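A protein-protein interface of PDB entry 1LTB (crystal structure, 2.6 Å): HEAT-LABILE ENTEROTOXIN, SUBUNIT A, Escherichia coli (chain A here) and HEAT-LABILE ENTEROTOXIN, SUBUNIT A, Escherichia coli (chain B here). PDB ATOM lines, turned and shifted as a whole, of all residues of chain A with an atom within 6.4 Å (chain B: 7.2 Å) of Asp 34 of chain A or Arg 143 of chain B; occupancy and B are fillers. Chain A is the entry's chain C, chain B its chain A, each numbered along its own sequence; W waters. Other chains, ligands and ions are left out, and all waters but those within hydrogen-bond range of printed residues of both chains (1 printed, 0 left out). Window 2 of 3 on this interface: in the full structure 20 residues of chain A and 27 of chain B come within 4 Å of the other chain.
NE of Arg 143 of chain B sits at hydrogen-bond distance from OE1 of Gln 30 of chain A (3.3 Å).
OD2 of Asp 34 of chain A is in salt-bridge range of NH2 of Arg 143 of chain B (3.0 Å).
O of Ser 119 of chain B lies within hydrogen-bond range of N of Arg 143 of chain B (3.2 Å).
Among the printed residues, pairs that only touch across the chains: Gln 30 of chain A with Tyr 146 of chain B and Ile 31 of chain A with Arg 143 of chain B.
Of chain B, only Arg 143 comes within 4 Å of Asp 34 of chain A.
Arg 143 of chain B touches just these residues of chain A: Gln 30 (3.3 Å), Ile 31 (3.5 Å) and Asp 34 (3.0 Å).
Of the printed residues of chain A, Tyr 146 of chain B touches Gln 30.
Of the printed residues of chain B, Ile 31 of chain A touches Arg 143 (3.5 Å).
Printed residues of chain B within 4 Å of Gln 30 of chain A: Arg 143 (3.3 Å) and Tyr 146 (3.4 Å).
Val 27 of chain A touches none of the printed residues of chain B.
The nearest printed residue of chain B that does not touch Asp 34 of chain A is Glu 141 of chain B (7.3 Å).
Printed residues of chain A that touch a printed residue of chain B: Gln 30, Ile 31 and Asp 34.
Among the printed residues, 4 pairs touch across the chains.
Water W1 lies within hydrogen-bond range of the side-chain amide nitrogen (NE2) of Gln 30 of chain A and the side-chain hydroxyl (OH) of Tyr 146 of chain B.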
ATOM      1  N   VAL A  27      23.709   7.033  18.433  1.00  0.00           N
ATOM      2  CA  VAL A  27      22.664   7.104  19.417  1.00  0.00           C
ATOM      3  C   VAL A  27      22.284   5.709  19.818  1.00  0.00           C
ATOM      4  O   VAL A  27      22.117   5.466  21.014  1.00  0.00           O
ATOM      5  CB  VAL A  27      21.427   7.843  18.863  1.00  0.00           C
ATOM      6  CG1 VAL A  27      20.140   7.665  19.693  1.00  0.00           C
ATOM      7  CG2 VAL A  27      21.796   9.297  18.940  1.00  0.00           C
ATOM      8  N   ARG A  29      24.103   3.001  19.605  1.00  0.00           N
ATOM      9  CA  ARG A  29      25.213   2.460  20.399  1.00  0.00           C
ATOM     10  C   ARG A  29      25.153   2.930  21.857  1.00  0.00           C
ATOM     11  O   ARG A  29      25.558   2.229  22.786  1.00  0.00           O
ATOM     12  CB  ARG A  29      26.512   2.884  19.750  1.00  0.00           C
ATOM     13  CG  ARG A  29      26.742   2.035  18.526  1.00  0.00           C
ATOM     14  CD  ARG A  29      27.847   2.538  17.630  1.00  0.00           C
ATOM     15  NE  ARG A  29      29.096   2.628  18.333  1.00  0.00           N
ATOM     16  CZ  ARG A  29      30.202   3.022  17.726  1.00  0.00           C
ATOM     17  NH1 ARG A  29      30.208   3.357  16.456  1.00  0.00           N
ATOM     18  NH2 ARG A  29      31.352   3.014  18.364  1.00  0.00           N
ATOM     19  N   GLN A  30      24.638   4.133  22.116  1.00  0.00           N
ATOM     20  CA  GLN A  30      24.447   4.645  23.450  1.00  0.00           C
ATOM     21  C   GLN A  30      23.350   3.931  24.215  1.00  0.00           C
ATOM     22  O   GLN A  30      23.645   3.299  25.234  1.00  0.00           O
ATOM     23  CB  GLN A  30      24.125   6.138  23.399  1.00  0.00           C
ATOM     24  CG  GLN A  30      25.358   6.986  23.217  1.00  0.00           C
ATOM     25  CD  GLN A  30      26.456   6.669  24.224  1.00  0.00           C
ATOM     26  OE1 GLN A  30      26.327   6.729  25.465  1.00  0.00           O
ATOM     27  NE2 GLN A  30      27.611   6.336  23.704  1.00  0.00           N
ATOM     28  N   ILE A  31      22.109   3.942  23.734  1.00  0.00           N
ATOM     29  CA  ILE A  31      20.964   3.423  24.463  1.00  0.00           C
ATOM     30  C   ILE A  31      20.812   1.894  24.422  1.00  0.00           C
ATOM     31  O   ILE A  31      20.483   1.247  25.421  1.00  0.00           O
ATOM     32  CB  ILE A  31      19.692   4.146  23.912  1.00  0.00           C
ATOM     33  CG1 ILE A  31      19.454   3.823  22.471  1.00  0.00           C
ATOM     34  CG2 ILE A  31      19.854   5.650  24.028  1.00  0.00           C
ATOM     35  CD1 ILE A  31      18.292   4.587  21.791  1.00  0.00           C
ATOM     36  N   PHE A  32      21.090   1.197  23.344  1.00  0.00           N
ATOM     37  CA  PHE A  32      20.896  -0.248  23.253  1.00  0.00           C
ATOM     38  C   PHE A  32      21.957  -0.980  23.991  1.00  0.00           C
ATOM     39  O   PHE A  32      21.701  -2.070  24.493  1.00  0.00           O
ATOM     40  CB  PHE A  32      20.894  -0.707  21.807  1.00  0.00           C
ATOM     41  CG  PHE A  32      19.643  -0.244  21.051  1.00  0.00           C
ATOM     42  CD1 PHE A  32      18.638   0.495  21.663  1.00  0.00           C
ATOM     43  CD2 PHE A  32      19.478  -0.611  19.726  1.00  0.00           C
ATOM     44  CE1 PHE A  32      17.502   0.841  20.960  1.00  0.00           C
ATOM     45  CE2 PHE A  32      18.334  -0.265  19.024  1.00  0.00           C
ATOM     46  CZ  PHE A  32      17.336   0.464  19.641  1.00  0.00           C
ATOM     47  N   SER A  33      23.096  -0.350  24.148  1.00  0.00           N
ATOM     48  CA  SER A  33      24.112  -0.929  24.957  1.00  0.00           C
ATOM     49  C   SER A  33      23.682  -1.081  26.397  1.00  0.00           C
ATOM     50  O   SER A  33      24.264  -1.887  27.119  1.00  0.00           O
ATOM     51  CB  SER A  33      25.329  -0.080  24.853  1.00  0.00           C
ATOM     52  OG  SER A  33      25.747  -0.257  23.496  1.00  0.00           O
ATOM     53  N   ASP A  34      22.596  -0.460  26.865  1.00  0.00           N
ATOM     54  CA  ASP A  34      22.155  -0.736  28.246  1.00  0.00           C
ATOM     55  C   ASP A  34      21.488  -2.091  28.445  1.00  0.00           C
ATOM     56  O   ASP A  34      21.275  -2.568  29.553  1.00  0.00           O
ATOM     57  CB  ASP A  34      21.208   0.370  28.688  1.00  0.00           C
ATOM     58  CG  ASP A  34      21.921   1.720  28.768  1.00  0.00           C
ATOM     59  OD1 ASP A  34      23.153   1.725  28.943  1.00  0.00           O
ATOM     60  OD2 ASP A  34      21.247   2.750  28.639  1.00  0.00           O
ATOM     61  N   TYR A  35      21.132  -2.714  27.333  1.00  0.00           N
ATOM     62  CA  TYR A  35      20.496  -3.992  27.388  1.00  0.00           C
ATOM     63  C   TYR A  35      21.501  -5.099  27.217  1.00  0.00           C
ATOM     64  O   TYR A  35      21.165  -6.264  27.437  1.00  0.00           O
ATOM     65  CB  TYR A  35      19.474  -4.062  26.305  1.00  0.00           C
ATOM     66  CG  TYR A  35      18.498  -2.917  26.413  1.00  0.00           C
ATOM     67  CD1 TYR A  35      17.651  -2.894  27.488  1.00  0.00           C
ATOM     68  CD2 TYR A  35      18.439  -1.931  25.466  1.00  0.00           C
ATOM     69  CE1 TYR A  35      16.726  -1.896  27.626  1.00  0.00           C
ATOM     70  CE2 TYR A  35      17.530  -0.908  25.588  1.00  0.00           C
ATOM     71  CZ  TYR A  35      16.675  -0.913  26.675  1.00  0.00           C
ATOM     72  OH  TYR A  35      15.716   0.053  26.855  1.00  0.00           O
ATOM     73  N   GLN A  36      22.747  -4.800  26.841  1.00  0.00           N
ATOM     74  CA  GLN A  36      23.644  -5.895  26.538  1.00  0.00           C
ATOM     75  C   GLN A  36      24.037  -6.618  27.795  1.00  0.00           C
ATOM     76  O   GLN A  36      24.475  -5.961  28.738  1.00  0.00           O
ATOM     77  CB  GLN A  36      24.857  -5.333  25.804  1.00  0.00           C
ATOM     78  CG  GLN A  36      26.118  -6.191  25.650  1.00  0.00           C
ATOM     79  CD  GLN A  36      25.978  -7.499  24.930  1.00  0.00           C
ATOM     80  OE1 GLN A  36      26.874  -8.330  25.023  1.00  0.00           O
ATOM     81  NE2 GLN A  36      24.922  -7.810  24.213  1.00  0.00           N
ATOM     82  N   SER A  37      23.855  -7.940  27.784  1.00  0.00           N
ATOM     83  CA  SER A  37      24.181  -8.744  28.925  1.00  0.00           C
ATOM     84  C   SER A  37      25.097  -9.838  28.432  1.00  0.00           C
ATOM     85  O   SER A  37      24.801 -10.677  27.557  1.00  0.00           O
ATOM     86  CB  SER A  37      22.937  -9.354  29.536  1.00  0.00           C
ATOM     87  OG  SER A  37      23.254  -9.837  30.846  1.00  0.00           O
ATOM     88  N   ALA B  86      21.508  19.515  24.651  1.00  0.00           N
ATOM     89  CA  ALA B  86      22.969  19.462  24.632  1.00  0.00           C
ATOM     90  C   ALA B  86      23.582  19.597  23.224  1.00  0.00           C
ATOM     91  O   ALA B  86      23.053  19.101  22.204  1.00  0.00           O
ATOM     92  CB  ALA B  86      23.419  18.143  25.221  1.00  0.00           C
ATOM     93  N   TYR B 118      15.680  12.114  22.280  1.00  0.00           N
ATOM     94  CA  TYR B 118      15.342  12.283  23.683  1.00  0.00           C
ATOM     95  C   TYR B 118      16.550  12.232  24.610  1.00  0.00           C
ATOM     96  O   TYR B 118      16.602  12.963  25.586  1.00  0.00           O
ATOM     97  CB  TYR B 118      14.327  11.215  24.073  1.00  0.00           C
ATOM     98  CG  TYR B 118      13.564  11.497  25.381  1.00  0.00           C
ATOM     99  CD1 TYR B 118      12.647  12.545  25.455  1.00  0.00           C
ATOM    100  CD2 TYR B 118      13.796  10.730  26.506  1.00  0.00           C
ATOM    101  CE1 TYR B 118      11.954  12.798  26.634  1.00  0.00           C
ATOM    102  CE2 TYR B 118      13.111  10.973  27.682  1.00  0.00           C
ATOM    103  CZ  TYR B 118      12.191  11.989  27.733  1.00  0.00           C
ATOM    104  OH  TYR B 118      11.490  12.195  28.882  1.00  0.00           O
ATOM    105  N   SER B 119      17.577  11.442  24.343  1.00  0.00           N
ATOM    106  CA  SER B 119      18.877  11.346  25.051  1.00  0.00           C
ATOM    107  C   SER B 119      19.729  12.629  25.124  1.00  0.00           C
ATOM    108  O   SER B 119      20.661  12.804  25.924  1.00  0.00           O
ATOM    109  CB  SER B 119      19.730  10.268  24.363  1.00  0.00           C
ATOM    110  OG  SER B 119      18.994   9.562  23.347  1.00  0.00           O
ATOM    111  N   GLN B 120      19.479  13.515  24.180  1.00  0.00           N
ATOM    112  CA  GLN B 120      20.200  14.747  24.049  1.00  0.00           C
ATOM    113  C   GLN B 120      19.457  15.823  24.808  1.00  0.00           C
ATOM    114  O   GLN B 120      20.072  16.857  25.041  1.00  0.00           O
ATOM    115  CB  GLN B 120      20.305  15.075  22.567  1.00  0.00           C
ATOM    116  CG  GLN B 120      21.471  15.945  22.181  1.00  0.00           C
ATOM    117  CD  GLN B 120      21.675  16.019  20.683  1.00  0.00           C
ATOM    118  OE1 GLN B 120      21.197  15.213  19.881  1.00  0.00           O
ATOM    119  NE2 GLN B 120      22.409  17.029  20.256  1.00  0.00           N
ATOM    120  N   ILE B 121      18.172  15.660  25.160  1.00  0.00           N
ATOM    121  CA  ILE B 121      17.419  16.631  25.939  1.00  0.00           C
ATOM    122  C   ILE B 121      17.815  16.559  27.402  1.00  0.00           C
ATOM    123  O   ILE B 121      17.607  15.595  28.157  1.00  0.00           O
ATOM    124  CB  ILE B 121      15.943  16.352  25.775  1.00  0.00           C
ATOM    125  CG1 ILE B 121      15.546  16.628  24.319  1.00  0.00           C
ATOM    126  CG2 ILE B 121      15.160  17.199  26.721  1.00  0.00           C
ATOM    127  CD1 ILE B 121      14.075  16.306  24.008  1.00  0.00           C
ATOM    128  N   TYR B 122      18.404  17.659  27.800  1.00  0.00           N
ATOM    129  CA  TYR B 122      18.843  17.715  29.168  1.00  0.00           C
ATOM    130  C   TYR B 122      17.673  17.906  30.157  1.00  0.00           C
ATOM    131  O   TYR B 122      17.695  17.406  31.274  1.00  0.00           O
ATOM    132  CB  TYR B 122      19.846  18.822  29.225  1.00  0.00           C
ATOM    133  CG  TYR B 122      20.317  19.007  30.636  1.00  0.00           C
ATOM    134  CD1 TYR B 122      21.373  18.270  31.060  1.00  0.00           C
ATOM    135  CD2 TYR B 122      19.705  19.929  31.460  1.00  0.00           C
ATOM    136  CE1 TYR B 122      21.864  18.437  32.315  1.00  0.00           C
ATOM    137  CE2 TYR B 122      20.201  20.096  32.729  1.00  0.00           C
ATOM    138  CZ  TYR B 122      21.283  19.349  33.130  1.00  0.00           C
ATOM    139  OH  TYR B 122      21.855  19.582  34.357  1.00  0.00           O
ATOM    140  N   ASN B 139      15.787  15.546  32.543  1.00  0.00           N
ATOM    141  CA  ASN B 139      15.504  14.369  31.779  1.00  0.00           C
ATOM    142  C   ASN B 139      16.473  13.338  32.296  1.00  0.00           C
ATOM    143  O   ASN B 139      17.663  13.399  32.051  1.00  0.00           O
ATOM    144  CB  ASN B 139      15.761  14.576  30.327  1.00  0.00           C
ATOM    145  CG  ASN B 139      15.425  13.345  29.518  1.00  0.00           C
ATOM    146  OD1 ASN B 139      14.934  12.326  29.998  1.00  0.00           O
ATOM    147  ND2 ASN B 139      15.727  13.352  28.242  1.00  0.00           N
ATOM    148  N   ARG B 140      15.979  12.344  33.011  1.00  0.00           N
ATOM    149  CA  ARG B 140      16.809  11.277  33.550  1.00  0.00           C
ATOM    150  C   ARG B 140      17.342  10.336  32.502  1.00  0.00           C
ATOM    151  O   ARG B 140      18.164   9.488  32.843  1.00  0.00           O
ATOM    152  CB  ARG B 140      16.050  10.417  34.568  1.00  0.00           C
ATOM    153  CG  ARG B 140      14.877   9.555  34.108  1.00  0.00           C
ATOM    154  CD  ARG B 140      13.585  10.347  33.997  1.00  0.00           C
ATOM    155  NE  ARG B 140      13.368  10.969  32.689  1.00  0.00           N
ATOM    156  CZ  ARG B 140      12.652  12.101  32.523  1.00  0.00           C
ATOM    157  NH1 ARG B 140      12.072  12.785  33.528  1.00  0.00           N
ATOM    158  NH2 ARG B 140      12.484  12.534  31.279  1.00  0.00           N
ATOM    159  N   GLU B 141      16.787  10.412  31.278  1.00  0.00           N
ATOM    160  CA  GLU B 141      17.264   9.604  30.165  1.00  0.00           C
ATOM    161  C   GLU B 141      18.387  10.222  29.355  1.00  0.00           C
ATOM    162  O   GLU B 141      18.869   9.600  28.393  1.00  0.00           O
ATOM    163  CB  GLU B 141      16.123   9.280  29.237  1.00  0.00           C
ATOM    164  CG  GLU B 141      15.415   8.179  29.971  1.00  0.00           C
ATOM    165  CD  GLU B 141      14.270   7.515  29.242  1.00  0.00           C
ATOM    166  OE1 GLU B 141      14.415   7.175  28.070  1.00  0.00           O
ATOM    167  OE2 GLU B 141      13.234   7.322  29.878  1.00  0.00           O
ATOM    168  N   TYR B 142      18.783  11.426  29.793  1.00  0.00           N
ATOM    169  CA  TYR B 142      19.852  12.209  29.211  1.00  0.00           C
ATOM    170  C   TYR B 142      21.158  11.435  29.409  1.00  0.00           C
ATOM    171  O   TYR B 142      21.334  10.786  30.443  1.00  0.00           O
ATOM    172  CB  TYR B 142      19.886  13.575  29.912  1.00  0.00           C
ATOM    173  CG  TYR B 142      21.089  14.437  29.549  1.00  0.00           C
ATOM    174  CD1 TYR B 142      21.281  14.966  28.280  1.00  0.00           C
ATOM    175  CD2 TYR B 142      22.014  14.656  30.539  1.00  0.00           C
ATOM    176  CE1 TYR B 142      22.417  15.712  28.000  1.00  0.00           C
ATOM    177  CE2 TYR B 142      23.147  15.400  30.268  1.00  0.00           C
ATOM    178  CZ  TYR B 142      23.353  15.920  29.006  1.00  0.00           C
ATOM    179  OH  TYR B 142      24.547  16.605  28.796  1.00  0.00           O
ATOM    180  N   ARG B 143      22.111  11.465  28.470  1.00  0.00           N
ATOM    181  CA  ARG B 143      23.280  10.634  28.628  1.00  0.00           C
ATOM    182  C   ARG B 143      24.426  11.527  28.837  1.00  0.00           C
ATOM    183  O   ARG B 143      25.203  11.916  27.954  1.00  0.00           O
ATOM    184  CB  ARG B 143      23.549   9.799  27.428  1.00  0.00           C
ATOM    185  CG  ARG B 143      22.370   8.942  27.243  1.00  0.00           C
ATOM    186  CD  ARG B 143      22.935   7.931  26.344  1.00  0.00           C
ATOM    187  NE  ARG B 143      23.488   6.829  27.110  1.00  0.00           N
ATOM    188  CZ  ARG B 143      22.735   5.811  27.490  1.00  0.00           C
ATOM    189  NH1 ARG B 143      21.427   5.708  27.194  1.00  0.00           N
ATOM    190  NH2 ARG B 143      23.348   4.919  28.251  1.00  0.00           N
ATOM    191  N   ASP B 144      24.548  11.731  30.121  1.00  0.00           N
ATOM    192  CA  ASP B 144      25.478  12.692  30.612  1.00  0.00           C
ATOM    193  C   ASP B 144      26.916  12.528  30.155  1.00  0.00           C
ATOM    194  O   ASP B 144      27.470  13.473  29.632  1.00  0.00           O
ATOM    195  CB  ASP B 144      25.360  12.665  32.123  1.00  0.00           C
ATOM    196  CG  ASP B 144      25.760  14.008  32.692  1.00  0.00           C
ATOM    197  OD1 ASP B 144      26.959  14.298  32.842  1.00  0.00           O
ATOM    198  OD2 ASP B 144      24.844  14.780  32.960  1.00  0.00           O
ATOM    199  N   ARG B 145      27.563  11.382  30.290  1.00  0.00           N
ATOM    200  CA  ARG B 145      28.971  11.212  29.923  1.00  0.00           C
ATOM    201  C   ARG B 145      29.123  11.397  28.429  1.00  0.00           C
ATOM    202  O   ARG B 145      30.158  11.920  28.012  1.00  0.00           O
ATOM    203  CB  ARG B 145      29.496   9.811  30.289  1.00  0.00           C
ATOM    204  CG  ARG B 145      31.016   9.561  30.021  1.00  0.00           C
ATOM    205  CD  ARG B 145      31.410   8.063  30.179  1.00  0.00           C
ATOM    206  NE  ARG B 145      31.250   7.739  31.585  1.00  0.00           N
ATOM    207  CZ  ARG B 145      30.430   6.852  32.152  1.00  0.00           C
ATOM    208  NH1 ARG B 145      29.591   6.056  31.512  1.00  0.00           N
ATOM    209  NH2 ARG B 145      30.330   6.889  33.466  1.00  0.00           N
ATOM    210  N   TYR B 146      28.079  11.048  27.653  1.00  0.00           N
ATOM    211  CA  TYR B 146      28.277  11.053  26.241  1.00  0.00           C
ATOM    212  C   TYR B 146      28.106  12.457  25.746  1.00  0.00           C
ATOM    213  O   TYR B 146      28.939  12.873  24.962  1.00  0.00           O
ATOM    214  CB  TYR B 146      27.302  10.117  25.560  1.00  0.00           C
ATOM    215  CG  TYR B 146      27.591   9.973  24.066  1.00  0.00           C
ATOM    216  CD1 TYR B 146      28.828   9.612  23.606  1.00  0.00           C
ATOM    217  CD2 TYR B 146      26.575  10.169  23.159  1.00  0.00           C
ATOM    218  CE1 TYR B 146      29.031   9.464  22.254  1.00  0.00           C
ATOM    219  CE2 TYR B 146      26.772  10.023  21.810  1.00  0.00           C
ATOM    220  CZ  TYR B 146      28.007   9.668  21.343  1.00  0.00           C
ATOM    221  OH  TYR B 146      28.208   9.510  19.959  1.00  0.00           O
ATOM    222  N   TYR B 147      27.098  13.240  26.119  1.00  0.00           N
ATOM    223  CA  TYR B 147      27.013  14.614  25.637  1.00  0.00           C
ATOM    224  C   TYR B 147      27.912  15.594  26.349  1.00  0.00           C
ATOM    225  O   TYR B 147      28.111  16.691  25.862  1.00  0.00           O
ATOM    226  CB  TYR B 147      25.605  15.099  25.730  1.00  0.00           C
ATOM    227  CG  TYR B 147      24.842  14.287  24.720  1.00  0.00           C
ATOM    228  CD1 TYR B 147      24.994  14.590  23.388  1.00  0.00           C
ATOM    229  CD2 TYR B 147      24.050  13.223  25.111  1.00  0.00           C
ATOM    230  CE1 TYR B 147      24.365  13.835  22.433  1.00  0.00           C
ATOM    231  CE2 TYR B 147      23.411  12.472  24.153  1.00  0.00           C
ATOM    232  CZ  TYR B 147      23.572  12.791  22.819  1.00  0.00           C
ATOM    233  OH  TYR B 147      22.884  12.097  21.832  1.00  0.00           O
ATOM    234  N   ARG B 148      28.558  15.199  27.427  1.00  0.00           N
ATOM    235  CA  ARG B 148      29.351  16.064  28.279  1.00  0.00           C
ATOM    236  C   ARG B 148      30.498  16.759  27.566  1.00  0.00           C
ATOM    237  O   ARG B 148      31.006  17.796  27.989  1.00  0.00           O
ATOM    238  CB  ARG B 148      29.871  15.200  29.426  1.00  0.00           C
ATOM    239  CG  ARG B 148      30.842  15.777  30.462  1.00  0.00           C
ATOM    240  CD  ARG B 148      31.309  14.721  31.469  1.00  0.00           C
ATOM    241  NE  ARG B 148      30.188  14.089  32.140  1.00  0.00           N
ATOM    242  CZ  ARG B 148      30.303  12.904  32.743  1.00  0.00           C
ATOM    243  NH1 ARG B 148      31.448  12.212  32.790  1.00  0.00           N
ATOM    244  NH2 ARG B 148      29.220  12.373  33.288  1.00  0.00           N
ATOM    245  N   LEU B 150      30.732  16.816  23.839  1.00  0.00           N
ATOM    246  CA  LEU B 150      30.386  17.100  22.482  1.00  0.00           C
ATOM    247  C   LEU B 150      29.935  18.528  22.371  1.00  0.00           C
ATOM    248  O   LEU B 150      29.412  19.181  23.283  1.00  0.00           O
ATOM    249  CB  LEU B 150      29.294  16.141  22.030  1.00  0.00           C
ATOM    250  CG  LEU B 150      29.574  14.635  22.202  1.00  0.00           C
ATOM    251  CD1 LEU B 150      28.334  13.843  21.848  1.00  0.00           C
ATOM    252  CD2 LEU B 150      30.718  14.189  21.325  1.00  0.00           C
HETATM  253  O   HOH W   1      28.029   6.219  20.850  1.00  0.00           O
